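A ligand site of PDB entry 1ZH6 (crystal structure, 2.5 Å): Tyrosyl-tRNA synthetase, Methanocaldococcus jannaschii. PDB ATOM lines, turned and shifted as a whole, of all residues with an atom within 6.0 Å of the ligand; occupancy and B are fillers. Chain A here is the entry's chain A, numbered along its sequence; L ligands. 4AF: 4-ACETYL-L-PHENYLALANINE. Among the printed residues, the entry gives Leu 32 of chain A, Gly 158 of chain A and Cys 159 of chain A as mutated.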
ATOM      1  N   LEU A  32       4.895  19.444   6.139  1.00  0.00           N
ATOM      2  CA  LEU A  32       5.749  19.562   4.979  1.00  0.00           C
ATOM      3  C   LEU A  32       6.812  18.458   5.024  1.00  0.00           C
ATOM      4  O   LEU A  32       7.322  18.124   6.065  1.00  0.00           O
ATOM      5  CB  LEU A  32       6.405  20.946   5.022  1.00  0.00           C
ATOM      6  CG  LEU A  32       7.672  21.185   4.232  1.00  0.00           C
ATOM      7  CD1 LEU A  32       7.343  21.000   2.799  1.00  0.00           C
ATOM      8  CD2 LEU A  32       8.201  22.593   4.490  1.00  0.00           C
ATOM      9  N   ILE A  33       7.094  17.885   3.885  1.00  0.00           N
ATOM     10  CA  ILE A  33       8.271  17.041   3.735  1.00  0.00           C
ATOM     11  C   ILE A  33       8.863  17.404   2.410  1.00  0.00           C
ATOM     12  O   ILE A  33       8.136  17.826   1.502  1.00  0.00           O
ATOM     13  CB  ILE A  33       7.917  15.518   3.765  1.00  0.00           C
ATOM     14  CG1 ILE A  33       9.176  14.661   3.881  1.00  0.00           C
ATOM     15  CG2 ILE A  33       7.095  15.118   2.557  1.00  0.00           C
ATOM     16  CD1 ILE A  33       8.909  13.236   4.308  1.00  0.00           C
ATOM     17  N   GLY A  34      10.184  17.247   2.301  1.00  0.00           N
ATOM     18  CA  GLY A  34      10.920  17.525   1.083  1.00  0.00           C
ATOM     19  C   GLY A  34      11.796  16.355   0.691  1.00  0.00           C
ATOM     20  O   GLY A  34      12.387  15.674   1.557  1.00  0.00           O
ATOM     21  N   PHE A  35      11.908  16.150  -0.620  1.00  0.00           N
ATOM     22  CA  PHE A  35      12.685  15.078  -1.207  1.00  0.00           C
ATOM     23  C   PHE A  35      13.480  15.582  -2.396  1.00  0.00           C
ATOM     24  O   PHE A  35      12.904  16.216  -3.272  1.00  0.00           O
ATOM     25  CB  PHE A  35      11.761  14.017  -1.798  1.00  0.00           C
ATOM     26  CG  PHE A  35      11.006  13.221  -0.800  1.00  0.00           C
ATOM     27  CD1 PHE A  35       9.630  13.332  -0.723  1.00  0.00           C
ATOM     28  CD2 PHE A  35      11.666  12.339   0.039  1.00  0.00           C
ATOM     29  CE1 PHE A  35       8.925  12.604   0.186  1.00  0.00           C
ATOM     30  CE2 PHE A  35      10.950  11.601   0.956  1.00  0.00           C
ATOM     31  CZ  PHE A  35       9.580  11.733   1.030  1.00  0.00           C
ATOM     32  N   GLU A  36      14.774  15.292  -2.446  1.00  0.00           N
ATOM     33  CA  GLU A  36      15.526  15.365  -3.685  1.00  0.00           C
ATOM     34  C   GLU A  36      14.940  14.290  -4.604  1.00  0.00           C
ATOM     35  O   GLU A  36      14.942  13.115  -4.234  1.00  0.00           O
ATOM     36  CB  GLU A  36      17.002  15.063  -3.462  1.00  0.00           C
ATOM     37  CG  GLU A  36      17.744  16.076  -2.613  1.00  0.00           C
ATOM     38  CD  GLU A  36      19.237  15.821  -2.613  1.00  0.00           C
ATOM     39  OE1 GLU A  36      19.778  15.441  -3.668  1.00  0.00           O
ATOM     40  OE2 GLU A  36      19.870  16.016  -1.538  1.00  0.00           O
ATOM     41  N   LEU A  65       7.516  19.011  -0.975  1.00  0.00           N
ATOM     42  CA  LEU A  65       8.522  19.823  -1.600  1.00  0.00           C
ATOM     43  C   LEU A  65       9.437  18.926  -2.398  1.00  0.00           C
ATOM     44  O   LEU A  65      10.226  18.126  -1.851  1.00  0.00           O
ATOM     45  CB  LEU A  65       9.285  20.620  -0.548  1.00  0.00           C
ATOM     46  CG  LEU A  65      10.354  21.575  -1.070  1.00  0.00           C
ATOM     47  CD1 LEU A  65       9.850  22.381  -2.235  1.00  0.00           C
ATOM     48  CD2 LEU A  65      10.773  22.504   0.077  1.00  0.00           C
ATOM     49  N   ALA A  67      12.412  18.803  -4.082  1.00  0.00           N
ATOM     50  CA  ALA A  67      13.538  19.683  -3.770  1.00  0.00           C
ATOM     51  C   ALA A  67      14.529  19.688  -4.931  1.00  0.00           C
ATOM     52  O   ALA A  67      15.560  19.030  -4.885  1.00  0.00           O
ATOM     53  CB  ALA A  67      14.185  19.216  -2.476  1.00  0.00           C
ATOM     54  N   HIS A  70      17.880  21.632  -4.309  1.00  0.00           N
ATOM     55  CA  HIS A  70      18.683  20.870  -3.367  1.00  0.00           C
ATOM     56  C   HIS A  70      19.385  19.772  -4.117  1.00  0.00           C
ATOM     57  O   HIS A  70      20.590  19.609  -3.971  1.00  0.00           O
ATOM     58  CB  HIS A  70      17.862  20.357  -2.188  1.00  0.00           C
ATOM     59  CG  HIS A  70      17.569  21.425  -1.184  1.00  0.00           C
ATOM     60  ND1 HIS A  70      16.469  22.238  -1.265  1.00  0.00           N
ATOM     61  CD2 HIS A  70      18.284  21.849  -0.114  1.00  0.00           C
ATOM     62  CE1 HIS A  70      16.501  23.107  -0.271  1.00  0.00           C
ATOM     63  NE2 HIS A  70      17.590  22.895   0.450  1.00  0.00           N
ATOM     64  N   PHE A 108       9.997  28.955  -5.436  1.00  0.00           N
ATOM     65  CA  PHE A 108      10.113  30.053  -4.481  1.00  0.00           C
ATOM     66  C   PHE A 108      11.518  30.232  -3.887  1.00  0.00           C
ATOM     67  O   PHE A 108      11.767  31.251  -3.256  1.00  0.00           O
ATOM     68  CB  PHE A 108       9.122  29.830  -3.344  1.00  0.00           C
ATOM     69  CG  PHE A 108       9.405  28.599  -2.526  1.00  0.00           C
ATOM     70  CD1 PHE A 108      10.126  28.680  -1.358  1.00  0.00           C
ATOM     71  CD2 PHE A 108       8.956  27.355  -2.957  1.00  0.00           C
ATOM     72  CE1 PHE A 108      10.416  27.543  -0.623  1.00  0.00           C
ATOM     73  CE2 PHE A 108       9.220  26.207  -2.223  1.00  0.00           C
ATOM     74  CZ  PHE A 108       9.951  26.313  -1.045  1.00  0.00           C
ATOM     75  N   GLN A 109      12.417  29.270  -4.087  1.00  0.00           N
ATOM     76  CA  GLN A 109      13.718  29.296  -3.421  1.00  0.00           C
ATOM     77  C   GLN A 109      14.761  30.183  -4.075  1.00  0.00           C
ATOM     78  O   GLN A 109      15.857  30.327  -3.537  1.00  0.00           O
ATOM     79  CB  GLN A 109      14.279  27.888  -3.273  1.00  0.00           C
ATOM     80  CG  GLN A 109      13.535  27.065  -2.244  1.00  0.00           C
ATOM     81  CD  GLN A 109      14.084  25.671  -2.155  1.00  0.00           C
ATOM     82  OE1 GLN A 109      14.477  25.098  -3.168  1.00  0.00           O
ATOM     83  NE2 GLN A 109      14.148  25.127  -0.958  1.00  0.00           N
ATOM     84  N   TYR A 114      14.033  35.320  -0.458  1.00  0.00           N
ATOM     85  CA  TYR A 114      14.453  34.010  -0.032  1.00  0.00           C
ATOM     86  C   TYR A 114      15.962  33.923  -0.009  1.00  0.00           C
ATOM     87  O   TYR A 114      16.534  33.410   0.950  1.00  0.00           O
ATOM     88  CB  TYR A 114      13.884  32.913  -0.941  1.00  0.00           C
ATOM     89  CG  TYR A 114      14.021  31.542  -0.333  1.00  0.00           C
ATOM     90  CD1 TYR A 114      12.956  30.944   0.302  1.00  0.00           C
ATOM     91  CD2 TYR A 114      15.227  30.852  -0.403  1.00  0.00           C
ATOM     92  CE1 TYR A 114      13.078  29.662   0.871  1.00  0.00           C
ATOM     93  CE2 TYR A 114      15.362  29.592   0.152  1.00  0.00           C
ATOM     94  CZ  TYR A 114      14.288  28.997   0.789  1.00  0.00           C
ATOM     95  OH  TYR A 114      14.409  27.734   1.334  1.00  0.00           O
ATOM     96  N   ILE A 137      24.022  13.225   3.943  1.00  0.00           N
ATOM     97  CA  ILE A 137      23.242  13.697   2.791  1.00  0.00           C
ATOM     98  C   ILE A 137      24.114  14.051   1.584  1.00  0.00           C
ATOM     99  O   ILE A 137      23.731  13.861   0.429  1.00  0.00           O
ATOM    100  CB  ILE A 137      22.459  14.951   3.191  1.00  0.00           C
ATOM    101  CG1 ILE A 137      21.353  14.601   4.174  1.00  0.00           C
ATOM    102  CG2 ILE A 137      21.869  15.645   1.960  1.00  0.00           C
ATOM    103  CD1 ILE A 137      20.915  15.795   5.022  1.00  0.00           C
ATOM    104  N   TYR A 151      23.421  24.212   0.674  1.00  0.00           N
ATOM    105  CA  TYR A 151      22.328  23.262   0.754  1.00  0.00           C
ATOM    106  C   TYR A 151      21.643  23.320   2.123  1.00  0.00           C
ATOM    107  O   TYR A 151      20.446  23.583   2.202  1.00  0.00           O
ATOM    108  CB  TYR A 151      22.887  21.877   0.442  1.00  0.00           C
ATOM    109  CG  TYR A 151      21.930  20.737   0.446  1.00  0.00           C
ATOM    110  CD1 TYR A 151      21.576  20.113  -0.738  1.00  0.00           C
ATOM    111  CD2 TYR A 151      21.381  20.241   1.645  1.00  0.00           C
ATOM    112  CE1 TYR A 151      20.730  19.021  -0.742  1.00  0.00           C
ATOM    113  CE2 TYR A 151      20.507  19.158   1.649  1.00  0.00           C
ATOM    114  CZ  TYR A 151      20.197  18.556   0.445  1.00  0.00           C
ATOM    115  OH  TYR A 151      19.336  17.482   0.407  1.00  0.00           O
ATOM    116  N   MET A 154      19.759  26.580   2.833  1.00  0.00           N
ATOM    117  CA  MET A 154      18.571  26.711   2.006  1.00  0.00           C
ATOM    118  C   MET A 154      17.462  25.845   2.516  1.00  0.00           C
ATOM    119  O   MET A 154      16.304  26.222   2.450  1.00  0.00           O
ATOM    120  CB  MET A 154      18.843  26.267   0.606  1.00  0.00           C
ATOM    121  CG  MET A 154      19.550  27.286  -0.195  1.00  0.00           C
ATOM    122  SD  MET A 154      18.625  27.509  -1.700  1.00  0.00           S
ATOM    123  CE  MET A 154      18.670  25.857  -2.426  1.00  0.00           C
ATOM    124  N   GLN A 155      17.810  24.623   2.935  1.00  0.00           N
ATOM    125  CA  GLN A 155      16.840  23.750   3.562  1.00  0.00           C
ATOM    126  C   GLN A 155      16.178  24.454   4.746  1.00  0.00           C
ATOM    127  O   GLN A 155      14.954  24.540   4.811  1.00  0.00           O
ATOM    128  CB  GLN A 155      17.497  22.447   4.011  1.00  0.00           C
ATOM    129  CG  GLN A 155      16.455  21.467   4.540  1.00  0.00           C
ATOM    130  CD  GLN A 155      16.861  20.045   4.421  1.00  0.00           C
ATOM    131  OE1 GLN A 155      17.687  19.670   3.567  1.00  0.00           O
ATOM    132  NE2 GLN A 155      16.282  19.216   5.271  1.00  0.00           N
ATOM    133  N   VAL A 156      17.001  24.996   5.641  1.00  0.00           N
ATOM    134  CA  VAL A 156      16.537  25.658   6.842  1.00  0.00           C
ATOM    135  C   VAL A 156      15.577  26.811   6.530  1.00  0.00           C
ATOM    136  O   VAL A 156      14.566  26.959   7.211  1.00  0.00           O
ATOM    137  CB  VAL A 156      17.720  26.182   7.687  1.00  0.00           C
ATOM    138  CG1 VAL A 156      17.230  27.037   8.852  1.00  0.00           C
ATOM    139  CG2 VAL A 156      18.547  25.028   8.226  1.00  0.00           C
ATOM    140  N   ASN A 157      15.896  27.609   5.522  1.00  0.00           N
ATOM    141  CA  ASN A 157      15.003  28.691   5.138  1.00  0.00           C
ATOM    142  C   ASN A 157      13.669  28.201   4.570  1.00  0.00           C
ATOM    143  O   ASN A 157      12.712  28.952   4.530  1.00  0.00           O
ATOM    144  CB  ASN A 157      15.667  29.651   4.134  1.00  0.00           C
ATOM    145  CG  ASN A 157      15.073  31.047   4.194  1.00  0.00           C
ATOM    146  OD1 ASN A 157      14.924  31.609   5.275  1.00  0.00           O
ATOM    147  ND2 ASN A 157      14.725  31.615   3.038  1.00  0.00           N
ATOM    148  N   GLY A 158      13.596  26.950   4.135  1.00  0.00           N
ATOM    149  CA  GLY A 158      12.353  26.415   3.556  1.00  0.00           C
ATOM    150  C   GLY A 158      11.443  25.689   4.541  1.00  0.00           C
ATOM    151  O   GLY A 158      10.323  25.307   4.192  1.00  0.00           O
ATOM    152  N   CYS A 159      11.907  25.492   5.765  1.00  0.00           N
ATOM    153  CA  CYS A 159      11.162  24.710   6.745  1.00  0.00           C
ATOM    154  C   CYS A 159       9.899  25.395   7.160  1.00  0.00           C
ATOM    155  O   CYS A 159       8.932  24.726   7.489  1.00  0.00           O
ATOM    156  CB  CYS A 159      12.017  24.406   7.977  1.00  0.00           C
ATOM    157  SG  CYS A 159      13.206  23.090   7.664  1.00  0.00           S
ATOM    158  N   HIS A 160       9.892  26.721   7.147  1.00  0.00           N
ATOM    159  CA  HIS A 160       8.725  27.489   7.537  1.00  0.00           C
ATOM    160  C   HIS A 160       7.779  27.765   6.363  1.00  0.00           C
ATOM    161  O   HIS A 160       6.927  28.669   6.446  1.00  0.00           O
ATOM    162  CB  HIS A 160       9.155  28.806   8.208  1.00  0.00           C
ATOM    163  CG  HIS A 160       9.851  29.809   7.304  1.00  0.00           C
ATOM    164  ND1 HIS A 160      11.189  29.734   6.975  1.00  0.00           N
ATOM    165  CD2 HIS A 160       9.385  30.959   6.742  1.00  0.00           C
ATOM    166  CE1 HIS A 160      11.518  30.777   6.229  1.00  0.00           C
ATOM    167  NE2 HIS A 160      10.441  31.530   6.065  1.00  0.00           N
ATOM    168  N   GLU A 172      18.336  11.255   9.222  1.00  0.00           N
ATOM    169  CA  GLU A 172      19.529  11.793   8.609  1.00  0.00           C
ATOM    170  C   GLU A 172      19.385  13.298   8.407  1.00  0.00           C
ATOM    171  O   GLU A 172      20.389  14.008   8.242  1.00  0.00           O
ATOM    172  CB  GLU A 172      19.880  11.084   7.285  1.00  0.00           C
ATOM    173  CG  GLU A 172      19.140  11.564   6.033  1.00  0.00           C
ATOM    174  CD  GLU A 172      17.690  11.131   5.996  1.00  0.00           C
ATOM    175  OE1 GLU A 172      17.294  10.278   6.830  1.00  0.00           O
ATOM    176  OE2 GLU A 172      16.949  11.648   5.129  1.00  0.00           O
ATOM    177  N   GLN A 173      18.138  13.779   8.408  1.00  0.00           N
ATOM    178  CA  GLN A 173      17.909  15.212   8.254  1.00  0.00           C
ATOM    179  C   GLN A 173      18.057  15.971   9.557  1.00  0.00           C
ATOM    180  O   GLN A 173      17.942  17.208   9.568  1.00  0.00           O
ATOM    181  CB  GLN A 173      16.496  15.470   7.720  1.00  0.00           C
ATOM    182  CG  GLN A 173      16.158  14.715   6.436  1.00  0.00           C
ATOM    183  CD  GLN A 173      16.878  15.233   5.199  1.00  0.00           C
ATOM    184  OE1 GLN A 173      16.943  16.436   4.962  1.00  0.00           O
ATOM    185  NE2 GLN A 173      17.390  14.318   4.377  1.00  0.00           N
ATOM    186  N   ILE A 176      20.430  19.160  10.278  1.00  0.00           N
ATOM    187  CA  ILE A 176      19.903  20.336   9.583  1.00  0.00           C
ATOM    188  C   ILE A 176      18.640  20.845  10.275  1.00  0.00           C
ATOM    189  O   ILE A 176      18.408  22.063  10.317  1.00  0.00           O
ATOM    190  CB  ILE A 176      19.553  20.031   8.093  1.00  0.00           C
ATOM    191  CG1 ILE A 176      20.781  19.643   7.292  1.00  0.00           C
ATOM    192  CG2 ILE A 176      18.943  21.253   7.397  1.00  0.00           C
ATOM    193  CD1 ILE A 176      20.475  19.305   5.880  1.00  0.00           C
ATOM    194  N   HIS A 177      17.824  19.933  10.798  1.00  0.00           N
ATOM    195  CA  HIS A 177      16.608  20.391  11.483  1.00  0.00           C
ATOM    196  C   HIS A 177      16.968  21.133  12.747  1.00  0.00           C
ATOM    197  O   HIS A 177      16.331  22.124  13.074  1.00  0.00           O
ATOM    198  CB  HIS A 177      15.661  19.242  11.766  1.00  0.00           C
ATOM    199  CG  HIS A 177      14.957  18.754  10.537  1.00  0.00           C
ATOM    200  ND1 HIS A 177      14.266  17.564  10.502  1.00  0.00           N
ATOM    201  CD2 HIS A 177      14.831  19.302   9.307  1.00  0.00           C
ATOM    202  CE1 HIS A 177      13.739  17.402   9.304  1.00  0.00           C
ATOM    203  NE2 HIS A 177      14.083  18.431   8.550  1.00  0.00           N
HETATM  204  C11 4AF L   1      12.426  22.664   3.603  1.00  0.00           C
HETATM  205  C8  4AF L   1      13.293  22.366   2.381  1.00  0.00           C
HETATM  206  O2  4AF L   1      13.635  23.262   1.617  1.00  0.00           O
HETATM  207  C7  4AF L   1      13.781  20.984   2.081  1.00  0.00           C
HETATM  208  C9  4AF L   1      14.499  20.856   0.907  1.00  0.00           C
HETATM  209  C10 4AF L   1      15.011  19.629   0.558  1.00  0.00           C
HETATM  210  C6  4AF L   1      13.577  19.898   2.932  1.00  0.00           C
HETATM  211  C5  4AF L   1      14.106  18.668   2.569  1.00  0.00           C
HETATM  212  C4  4AF L   1      14.826  18.553   1.389  1.00  0.00           C
HETATM  213  C3  4AF L   1      15.394  17.232   0.916  1.00  0.00           C
HETATM  214  CA  4AF L   1      16.250  16.569   1.935  1.00  0.00           C
HETATM  215  C   4AF L   1      16.755  15.261   1.303  1.00  0.00           C
HETATM  216  OXT 4AF L   1      17.838  14.789   1.635  1.00  0.00           O
HETATM  217  O   4AF L   1      16.086  14.651   0.455  1.00  0.00           O
HETATM  218  N   4AF L   1      17.364  17.474   2.258  1.00  0.00           N
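Gly 34 touches the ligand (O to C3, 3.4 Å). Phe 35 touches the ligand (CA to O, 3.8 Å). CD2 of Leu 65 touches O2 of the ligand, at 3.3 Å. Ala 67 touches the ligand. His 70 touches the ligand. Gly 158 touches the ligand. Cys 159 touches the ligand. Of the 24 residues printed, 12 come within 4 Å of the ligand.
The side-chain amide oxygen (OE1) of Gln 173 lies within hydrogen-bond range of the side-chain amide nitrogen (NE2) of Gln 155 (2.9 Å). A ring nitrogen (NE2) of His 70 is in hydrogen-bond range of the backbone NH (N) of Gln 155, at 3.0 Å. The backbone carbonyl oxygen (O) of Tyr 151 lies within hydrogen-bond range of a ring nitrogen (NE2) of His 70 (3.4 Å). OE2 of Glu 36 sits at hydrogen-bond distance from OH of Tyr 151 (2.5 Å). The side-chain amide nitrogen (NE2) of Gln 173 sits at hydrogen-bond distance from the side-chain carboxylate (OE2) of Glu 172, 2.8 Å away. The side-chain amide nitrogen (NE2) of Gln 109 is in hydrogen-bond range of the side-chain hydroxyl (OH) of Tyr 114 (3.5 Å). The side-chain hydroxyl (OH) of Tyr 114 sits at hydrogen-bond distance from the backbone NH (N) of Gly 158 (3.0 Å). O of Leu 65 is in hydrogen-bond range of N of Phe 35, at 2.9 Å.
A nitrogen (N) of the ligand is in hydrogen-bond range of the side-chain amide oxygen of Gln 155 (2.6 Å). N of the ligand sits at hydrogen-bond distance from OH of Tyr 151 (2.7 Å). An oxygen (OXT) of the ligand is in hydrogen-bond range of the side-chain amide nitrogen of Gln 173 (2.8 Å). NE2 of Gln 109 sits at hydrogen-bond distance from O2 of the ligand (3.2 Å). The backbone NH (N) of Glu 36 is in hydrogen-bond range of an oxygen (O) of the ligand (3.2 Å).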
